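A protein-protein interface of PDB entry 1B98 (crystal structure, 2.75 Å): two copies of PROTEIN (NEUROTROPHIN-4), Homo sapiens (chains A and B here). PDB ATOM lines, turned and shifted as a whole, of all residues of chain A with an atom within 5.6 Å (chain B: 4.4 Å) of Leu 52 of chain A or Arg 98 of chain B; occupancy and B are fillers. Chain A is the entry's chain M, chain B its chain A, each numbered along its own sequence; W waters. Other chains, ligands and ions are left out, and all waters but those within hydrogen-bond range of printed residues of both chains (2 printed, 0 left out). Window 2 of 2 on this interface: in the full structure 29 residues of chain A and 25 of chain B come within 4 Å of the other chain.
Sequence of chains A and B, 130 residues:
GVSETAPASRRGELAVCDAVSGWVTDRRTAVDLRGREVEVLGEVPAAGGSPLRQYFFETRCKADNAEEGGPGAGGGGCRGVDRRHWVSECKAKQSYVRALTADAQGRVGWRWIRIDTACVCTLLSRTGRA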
ATOM      1  N   GLY A  42     -20.455  25.887 -32.937  1.00  0.00           N
ATOM      2  CA  GLY A  42     -21.869  25.901 -32.630  1.00  0.00           C
ATOM      3  C   GLY A  42     -22.390  24.487 -32.591  1.00  0.00           C
ATOM      4  O   GLY A  42     -23.277  24.120 -31.803  1.00  0.00           O
ATOM      5  N   GLU A  43     -21.785  23.641 -33.445  1.00  0.00           N
ATOM      6  CA  GLU A  43     -22.181  22.228 -33.520  1.00  0.00           C
ATOM      7  C   GLU A  43     -21.106  21.203 -33.205  1.00  0.00           C
ATOM      8  O   GLU A  43     -19.901  21.362 -33.310  1.00  0.00           O
ATOM      9  CB  GLU A  43     -22.790  21.897 -34.890  1.00  0.00           C
ATOM     10  CG  GLU A  43     -23.920  22.791 -35.355  1.00  0.00           C
ATOM     11  CD  GLU A  43     -24.654  22.474 -36.645  1.00  0.00           C
ATOM     12  OE1 GLU A  43     -24.626  21.326 -37.161  1.00  0.00           O
ATOM     13  OE2 GLU A  43     -25.325  23.408 -37.169  1.00  0.00           O
ATOM     14  N   VAL A  44     -21.546  20.040 -32.746  1.00  0.00           N
ATOM     15  CA  VAL A  44     -20.784  18.886 -32.360  1.00  0.00           C
ATOM     16  C   VAL A  44     -21.417  17.706 -33.094  1.00  0.00           C
ATOM     17  O   VAL A  44     -22.509  17.246 -32.769  1.00  0.00           O
ATOM     18  CB  VAL A  44     -20.725  18.570 -30.863  1.00  0.00           C
ATOM     19  CG1 VAL A  44     -20.095  17.193 -30.626  1.00  0.00           C
ATOM     20  CG2 VAL A  44     -19.966  19.612 -30.064  1.00  0.00           C
ATOM     21  N   PRO A  45     -20.655  17.173 -34.045  1.00  0.00           N
ATOM     22  CA  PRO A  45     -21.166  16.092 -34.870  1.00  0.00           C
ATOM     23  C   PRO A  45     -21.321  14.726 -34.246  1.00  0.00           C
ATOM     24  O   PRO A  45     -22.318  14.064 -34.560  1.00  0.00           O
ATOM     25  CB  PRO A  45     -20.216  16.055 -36.052  1.00  0.00           C
ATOM     26  CG  PRO A  45     -19.021  16.851 -35.703  1.00  0.00           C
ATOM     27  CD  PRO A  45     -19.335  17.649 -34.480  1.00  0.00           C
ATOM     28  N   ALA A  47     -20.222  13.448 -30.624  1.00  0.00           N
ATOM     29  CA  ALA A  47     -19.798  13.426 -29.239  1.00  0.00           C
ATOM     30  C   ALA A  47     -21.072  12.959 -28.517  1.00  0.00           C
ATOM     31  O   ALA A  47     -22.014  13.691 -28.276  1.00  0.00           O
ATOM     32  CB  ALA A  47     -19.317  14.727 -28.679  1.00  0.00           C
ATOM     33  N   SER A  50     -24.863  10.334 -30.666  1.00  0.00           N
ATOM     34  CA  SER A  50     -25.537  11.301 -31.478  1.00  0.00           C
ATOM     35  C   SER A  50     -24.862  12.669 -31.547  1.00  0.00           C
ATOM     36  O   SER A  50     -23.982  13.090 -30.811  1.00  0.00           O
ATOM     37  CB  SER A  50     -26.973  11.508 -30.940  1.00  0.00           C
ATOM     38  OG  SER A  50     -27.995  10.836 -31.643  1.00  0.00           O
ATOM     39  N   PRO A  51     -25.335  13.412 -32.538  1.00  0.00           N
ATOM     40  CA  PRO A  51     -24.914  14.772 -32.825  1.00  0.00           C
ATOM     41  C   PRO A  51     -25.654  15.755 -31.929  1.00  0.00           C
ATOM     42  O   PRO A  51     -26.747  15.440 -31.441  1.00  0.00           O
ATOM     43  CB  PRO A  51     -25.261  14.946 -34.295  1.00  0.00           C
ATOM     44  CG  PRO A  51     -25.729  13.610 -34.789  1.00  0.00           C
ATOM     45  CD  PRO A  51     -26.350  13.004 -33.548  1.00  0.00           C
ATOM     46  N   LEU A  52     -25.072  16.910 -31.633  1.00  0.00           N
ATOM     47  CA  LEU A  52     -25.729  17.885 -30.788  1.00  0.00           C
ATOM     48  C   LEU A  52     -25.168  19.297 -30.906  1.00  0.00           C
ATOM     49  O   LEU A  52     -24.096  19.535 -31.425  1.00  0.00           O
ATOM     50  CB  LEU A  52     -25.735  17.465 -29.329  1.00  0.00           C
ATOM     51  CG  LEU A  52     -24.494  17.538 -28.466  1.00  0.00           C
ATOM     52  CD1 LEU A  52     -24.774  16.893 -27.112  1.00  0.00           C
ATOM     53  CD2 LEU A  52     -23.293  16.888 -29.120  1.00  0.00           C
ATOM     54  N   ARG A  53     -25.974  20.214 -30.384  1.00  0.00           N
ATOM     55  CA  ARG A  53     -25.711  21.634 -30.345  1.00  0.00           C
ATOM     56  C   ARG A  53     -24.775  21.938 -29.176  1.00  0.00           C
ATOM     57  O   ARG A  53     -24.912  21.383 -28.109  1.00  0.00           O
ATOM     58  CB  ARG A  53     -27.008  22.432 -30.310  1.00  0.00           C
ATOM     59  CG  ARG A  53     -26.983  23.846 -29.750  1.00  0.00           C
ATOM     60  CD  ARG A  53     -27.834  24.744 -30.617  1.00  0.00           C
ATOM     61  NE  ARG A  53     -28.090  26.095 -30.138  1.00  0.00           N
ATOM     62  CZ  ARG A  53     -28.489  27.025 -31.017  1.00  0.00           C
ATOM     63  NH1 ARG A  53     -28.637  26.701 -32.297  1.00  0.00           N
ATOM     64  NH2 ARG A  53     -28.743  28.270 -30.663  1.00  0.00           N
ATOM     65  N   GLN A  54     -23.712  22.721 -29.447  1.00  0.00           N
ATOM     66  CA  GLN A  54     -22.805  23.055 -28.352  1.00  0.00           C
ATOM     67  C   GLN A  54     -23.256  24.338 -27.649  1.00  0.00           C
ATOM     68  O   GLN A  54     -23.256  25.383 -28.300  1.00  0.00           O
ATOM     69  CB  GLN A  54     -21.352  23.209 -28.793  1.00  0.00           C
ATOM     70  CG  GLN A  54     -20.365  23.514 -27.693  1.00  0.00           C
ATOM     71  CD  GLN A  54     -18.943  23.137 -28.111  1.00  0.00           C
ATOM     72  OE1 GLN A  54     -18.313  22.271 -27.530  1.00  0.00           O
ATOM     73  NE2 GLN A  54     -18.347  23.780 -29.096  1.00  0.00           N
ATOM     74  N   TYR A  55     -23.556  24.273 -26.379  1.00  0.00           N
ATOM     75  CA  TYR A  55     -23.841  25.438 -25.570  1.00  0.00           C
ATOM     76  C   TYR A  55     -23.346  25.242 -24.136  1.00  0.00           C
ATOM     77  O   TYR A  55     -22.667  24.306 -23.712  1.00  0.00           O
ATOM     78  CB  TYR A  55     -25.282  25.971 -25.673  1.00  0.00           C
ATOM     79  CG  TYR A  55     -26.204  24.879 -25.164  1.00  0.00           C
ATOM     80  CD1 TYR A  55     -26.596  23.828 -25.967  1.00  0.00           C
ATOM     81  CD2 TYR A  55     -26.610  24.934 -23.844  1.00  0.00           C
ATOM     82  CE1 TYR A  55     -27.383  22.818 -25.446  1.00  0.00           C
ATOM     83  CE2 TYR A  55     -27.419  23.947 -23.324  1.00  0.00           C
ATOM     84  CZ  TYR A  55     -27.805  22.884 -24.117  1.00  0.00           C
ATOM     85  OH  TYR A  55     -28.614  21.910 -23.563  1.00  0.00           O
ATOM     86  N   PHE B  56     -13.518  17.060 -14.904  1.00  0.00           N
ATOM     87  CA  PHE B  56     -14.155  18.329 -14.626  1.00  0.00           C
ATOM     88  C   PHE B  56     -13.195  19.270 -13.889  1.00  0.00           C
ATOM     89  O   PHE B  56     -12.392  18.878 -13.030  1.00  0.00           O
ATOM     90  CB  PHE B  56     -15.432  18.287 -13.746  1.00  0.00           C
ATOM     91  CG  PHE B  56     -16.330  17.208 -14.291  1.00  0.00           C
ATOM     92  CD1 PHE B  56     -17.094  17.466 -15.430  1.00  0.00           C
ATOM     93  CD2 PHE B  56     -16.232  15.918 -13.782  1.00  0.00           C
ATOM     94  CE1 PHE B  56     -17.866  16.457 -15.962  1.00  0.00           C
ATOM     95  CE2 PHE B  56     -17.009  14.920 -14.335  1.00  0.00           C
ATOM     96  CZ  PHE B  56     -17.836  15.195 -15.417  1.00  0.00           C
ATOM     97  N   TYR B  96     -23.607  24.451 -14.144  1.00  0.00           N
ATOM     98  CA  TYR B  96     -23.902  23.178 -14.803  1.00  0.00           C
ATOM     99  C   TYR B  96     -22.833  22.851 -15.829  1.00  0.00           C
ATOM    100  O   TYR B  96     -22.392  23.714 -16.581  1.00  0.00           O
ATOM    101  CB  TYR B  96     -25.318  23.317 -15.397  1.00  0.00           C
ATOM    102  CG  TYR B  96     -26.430  23.164 -14.358  1.00  0.00           C
ATOM    103  CD1 TYR B  96     -26.840  21.901 -13.954  1.00  0.00           C
ATOM    104  CD2 TYR B  96     -27.051  24.290 -13.803  1.00  0.00           C
ATOM    105  CE1 TYR B  96     -27.838  21.768 -13.023  1.00  0.00           C
ATOM    106  CE2 TYR B  96     -28.056  24.168 -12.873  1.00  0.00           C
ATOM    107  CZ  TYR B  96     -28.440  22.892 -12.485  1.00  0.00           C
ATOM    108  OH  TYR B  96     -29.445  22.742 -11.543  1.00  0.00           O
ATOM    109  N   VAL B  97     -22.359  21.615 -15.894  1.00  0.00           N
ATOM    110  CA  VAL B  97     -21.412  21.204 -16.926  1.00  0.00           C
ATOM    111  C   VAL B  97     -22.065  20.013 -17.612  1.00  0.00           C
ATOM    112  O   VAL B  97     -22.837  19.279 -17.019  1.00  0.00           O
ATOM    113  CB  VAL B  97     -19.956  20.979 -16.535  1.00  0.00           C
ATOM    114  CG1 VAL B  97     -19.450  22.276 -15.864  1.00  0.00           C
ATOM    115  CG2 VAL B  97     -19.695  19.863 -15.558  1.00  0.00           C
ATOM    116  N   ARG B  98     -21.860  19.930 -18.910  1.00  0.00           N
ATOM    117  CA  ARG B  98     -22.309  18.871 -19.776  1.00  0.00           C
ATOM    118  C   ARG B  98     -21.513  17.612 -19.380  1.00  0.00           C
ATOM    119  O   ARG B  98     -20.280  17.680 -19.403  1.00  0.00           O
ATOM    120  CB  ARG B  98     -21.909  19.128 -21.227  1.00  0.00           C
ATOM    121  CG  ARG B  98     -22.897  19.708 -22.189  1.00  0.00           C
ATOM    122  CD  ARG B  98     -24.071  18.898 -22.691  1.00  0.00           C
ATOM    123  NE  ARG B  98     -24.353  19.373 -24.008  1.00  0.00           N
ATOM    124  CZ  ARG B  98     -25.240  19.427 -24.967  1.00  0.00           C
ATOM    125  NH1 ARG B  98     -24.959  20.044 -26.122  1.00  0.00           N
ATOM    126  NH2 ARG B  98     -26.425  18.867 -24.837  1.00  0.00           N
ATOM    127  N   ALA B  99     -22.192  16.512 -19.080  1.00  0.00           N
ATOM    128  CA  ALA B  99     -21.460  15.312 -18.714  1.00  0.00           C
ATOM    129  C   ALA B  99     -22.092  14.045 -19.257  1.00  0.00           C
ATOM    130  O   ALA B  99     -23.287  13.864 -19.515  1.00  0.00           O
ATOM    131  CB  ALA B  99     -21.284  15.344 -17.203  1.00  0.00           C
ATOM    132  N   TRP B 110     -25.605  12.574 -22.467  1.00  0.00           N
ATOM    133  CA  TRP B 110     -25.152  13.880 -22.030  1.00  0.00           C
ATOM    134  C   TRP B 110     -26.249  14.558 -21.209  1.00  0.00           C
ATOM    135  O   TRP B 110     -27.395  14.664 -21.600  1.00  0.00           O
ATOM    136  CB  TRP B 110     -24.710  14.860 -23.122  1.00  0.00           C
ATOM    137  CG  TRP B 110     -23.630  14.199 -23.928  1.00  0.00           C
ATOM    138  CD1 TRP B 110     -23.854  13.487 -25.074  1.00  0.00           C
ATOM    139  CD2 TRP B 110     -22.245  14.080 -23.620  1.00  0.00           C
ATOM    140  NE1 TRP B 110     -22.674  12.926 -25.482  1.00  0.00           N
ATOM    141  CE2 TRP B 110     -21.662  13.292 -24.638  1.00  0.00           C
ATOM    142  CE3 TRP B 110     -21.413  14.592 -22.631  1.00  0.00           C
ATOM    143  CZ2 TRP B 110     -20.301  12.986 -24.675  1.00  0.00           C
ATOM    144  CZ3 TRP B 110     -20.062  14.275 -22.633  1.00  0.00           C
ATOM    145  CH2 TRP B 110     -19.520  13.472 -23.653  1.00  0.00           C
ATOM    146  N   ARG B 111     -25.858  14.858 -19.980  1.00  0.00           N
ATOM    147  CA  ARG B 111     -26.696  15.542 -19.034  1.00  0.00           C
ATOM    148  C   ARG B 111     -25.881  16.683 -18.388  1.00  0.00           C
ATOM    149  O   ARG B 111     -24.661  16.648 -18.116  1.00  0.00           O
ATOM    150  CB  ARG B 111     -27.267  14.674 -17.920  1.00  0.00           C
ATOM    151  CG  ARG B 111     -28.133  13.486 -18.308  1.00  0.00           C
ATOM    152  CD  ARG B 111     -28.413  12.657 -17.035  1.00  0.00           C
ATOM    153  NE  ARG B 111     -28.363  11.247 -17.435  1.00  0.00           N
ATOM    154  CZ  ARG B 111     -29.395  10.580 -17.921  1.00  0.00           C
ATOM    155  NH1 ARG B 111     -30.551  11.219 -17.987  1.00  0.00           N
ATOM    156  NH2 ARG B 111     -29.284   9.334 -18.333  1.00  0.00           N
ATOM    157  N   TRP B 112     -26.669  17.712 -18.100  1.00  0.00           N
ATOM    158  CA  TRP B 112     -26.137  18.841 -17.372  1.00  0.00           C
ATOM    159  C   TRP B 112     -25.964  18.449 -15.923  1.00  0.00           C
ATOM    160  O   TRP B 112     -26.961  18.052 -15.382  1.00  0.00           O
ATOM    161  CB  TRP B 112     -27.111  19.992 -17.596  1.00  0.00           C
ATOM    162  CG  TRP B 112     -26.957  20.421 -19.042  1.00  0.00           C
ATOM    163  CD1 TRP B 112     -27.738  20.138 -20.108  1.00  0.00           C
ATOM    164  CD2 TRP B 112     -25.893  21.282 -19.517  1.00  0.00           C
ATOM    165  NE1 TRP B 112     -27.234  20.778 -21.223  1.00  0.00           N
ATOM    166  CE2 TRP B 112     -26.108  21.475 -20.902  1.00  0.00           C
ATOM    167  CE3 TRP B 112     -24.802  21.902 -18.913  1.00  0.00           C
ATOM    168  CZ2 TRP B 112     -25.272  22.286 -21.683  1.00  0.00           C
ATOM    169  CZ3 TRP B 112     -23.963  22.665 -19.692  1.00  0.00           C
ATOM    170  CH2 TRP B 112     -24.185  22.865 -21.071  1.00  0.00           C
HETATM  171  O   HOH W   1     -29.709  19.657 -24.921  1.00  0.00           O
HETATM  172  O   HOH W   2     -22.500  21.275 -25.433  1.00  0.00           O
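The side-chain hydroxyl (OH) of Tyr 55 of chain A sits at hydrogen-bond distance from the indole nitrogen (NE1) of Trp 112 of chain B (2.9 Å).
The guanidinium group (NH1) of Arg 98 of chain B sits close to the backbone carbonyl oxygen (O) of Arg 53 of chain A (2.4 Å).
O of Ala 47 of chain A lies within hydrogen-bond range of NE1 of Trp 110 of chain B (3.0 Å).
N of Leu 52 of chain A sits at hydrogen-bond distance from O of Val 44 of chain A (2.8 Å).
NH1 of Arg 98 of chain B touches CD1 of Leu 52 of chain A, at 3.3 Å.
NH1 of Arg 98 of chain B touches CE1 of Tyr 55 of chain A, 3.7 Å away.
Of chain B, only Arg 98 (3.3 Å) comes within 4 Å of Leu 52 of chain A.
Arg 98 of chain B touches just these residues of chain A: Leu 52, Arg 53 and Tyr 55.
Of the printed residues of chain B, Ala 47 of chain A touches Trp 110 (3.0 Å).
Of the printed residues of chain B, Arg 53 of chain A touches Arg 98.
Pro 51 of chain A touches none of the printed residues of chain B.
Gly 42 of chain A touches none of the printed residues of chain B.
The nearest residue of chain A that does not touch Arg 98 of chain B is Gln 54 of chain A (4.3 Å).
The nearest printed residue of chain A that does not touch Trp 112 of chain B is Arg 53 of chain A (6.5 Å).
Printed residues of chain A that touch a printed residue of chain B: Ala 47, Leu 52, Arg 53 and Tyr 55.
Of the 8 printed residues of chain B, 3 touch a printed residue of chain A.
Printed residues of chain B that touch a printed residue of chain A: Arg 98, Trp 110 and Trp 112.
Hydrophobic or aromatic side chains of chain B within 4 Å of the printed part of chain A: Trp 110 and Trp 112.
Among the printed residues, 5 pairs touch across the chains.
Among the printed residues, no Asp or Glu carboxylate lies within 4 Å of a Lys or Arg side-chain nitrogen of the other chain.
No position is printed for both chains.
Water W2 bridges the guanidinium group (NH1) of Arg 98 of chain B (2.8 Å) and the backbone NH (N) of Tyr 55 of chain A (3.3 Å).
Water W1 lies within hydrogen-bond range of the side-chain hydroxyl of Tyr 55 of chain A and the guanidinium group of Arg 98 of chain B.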
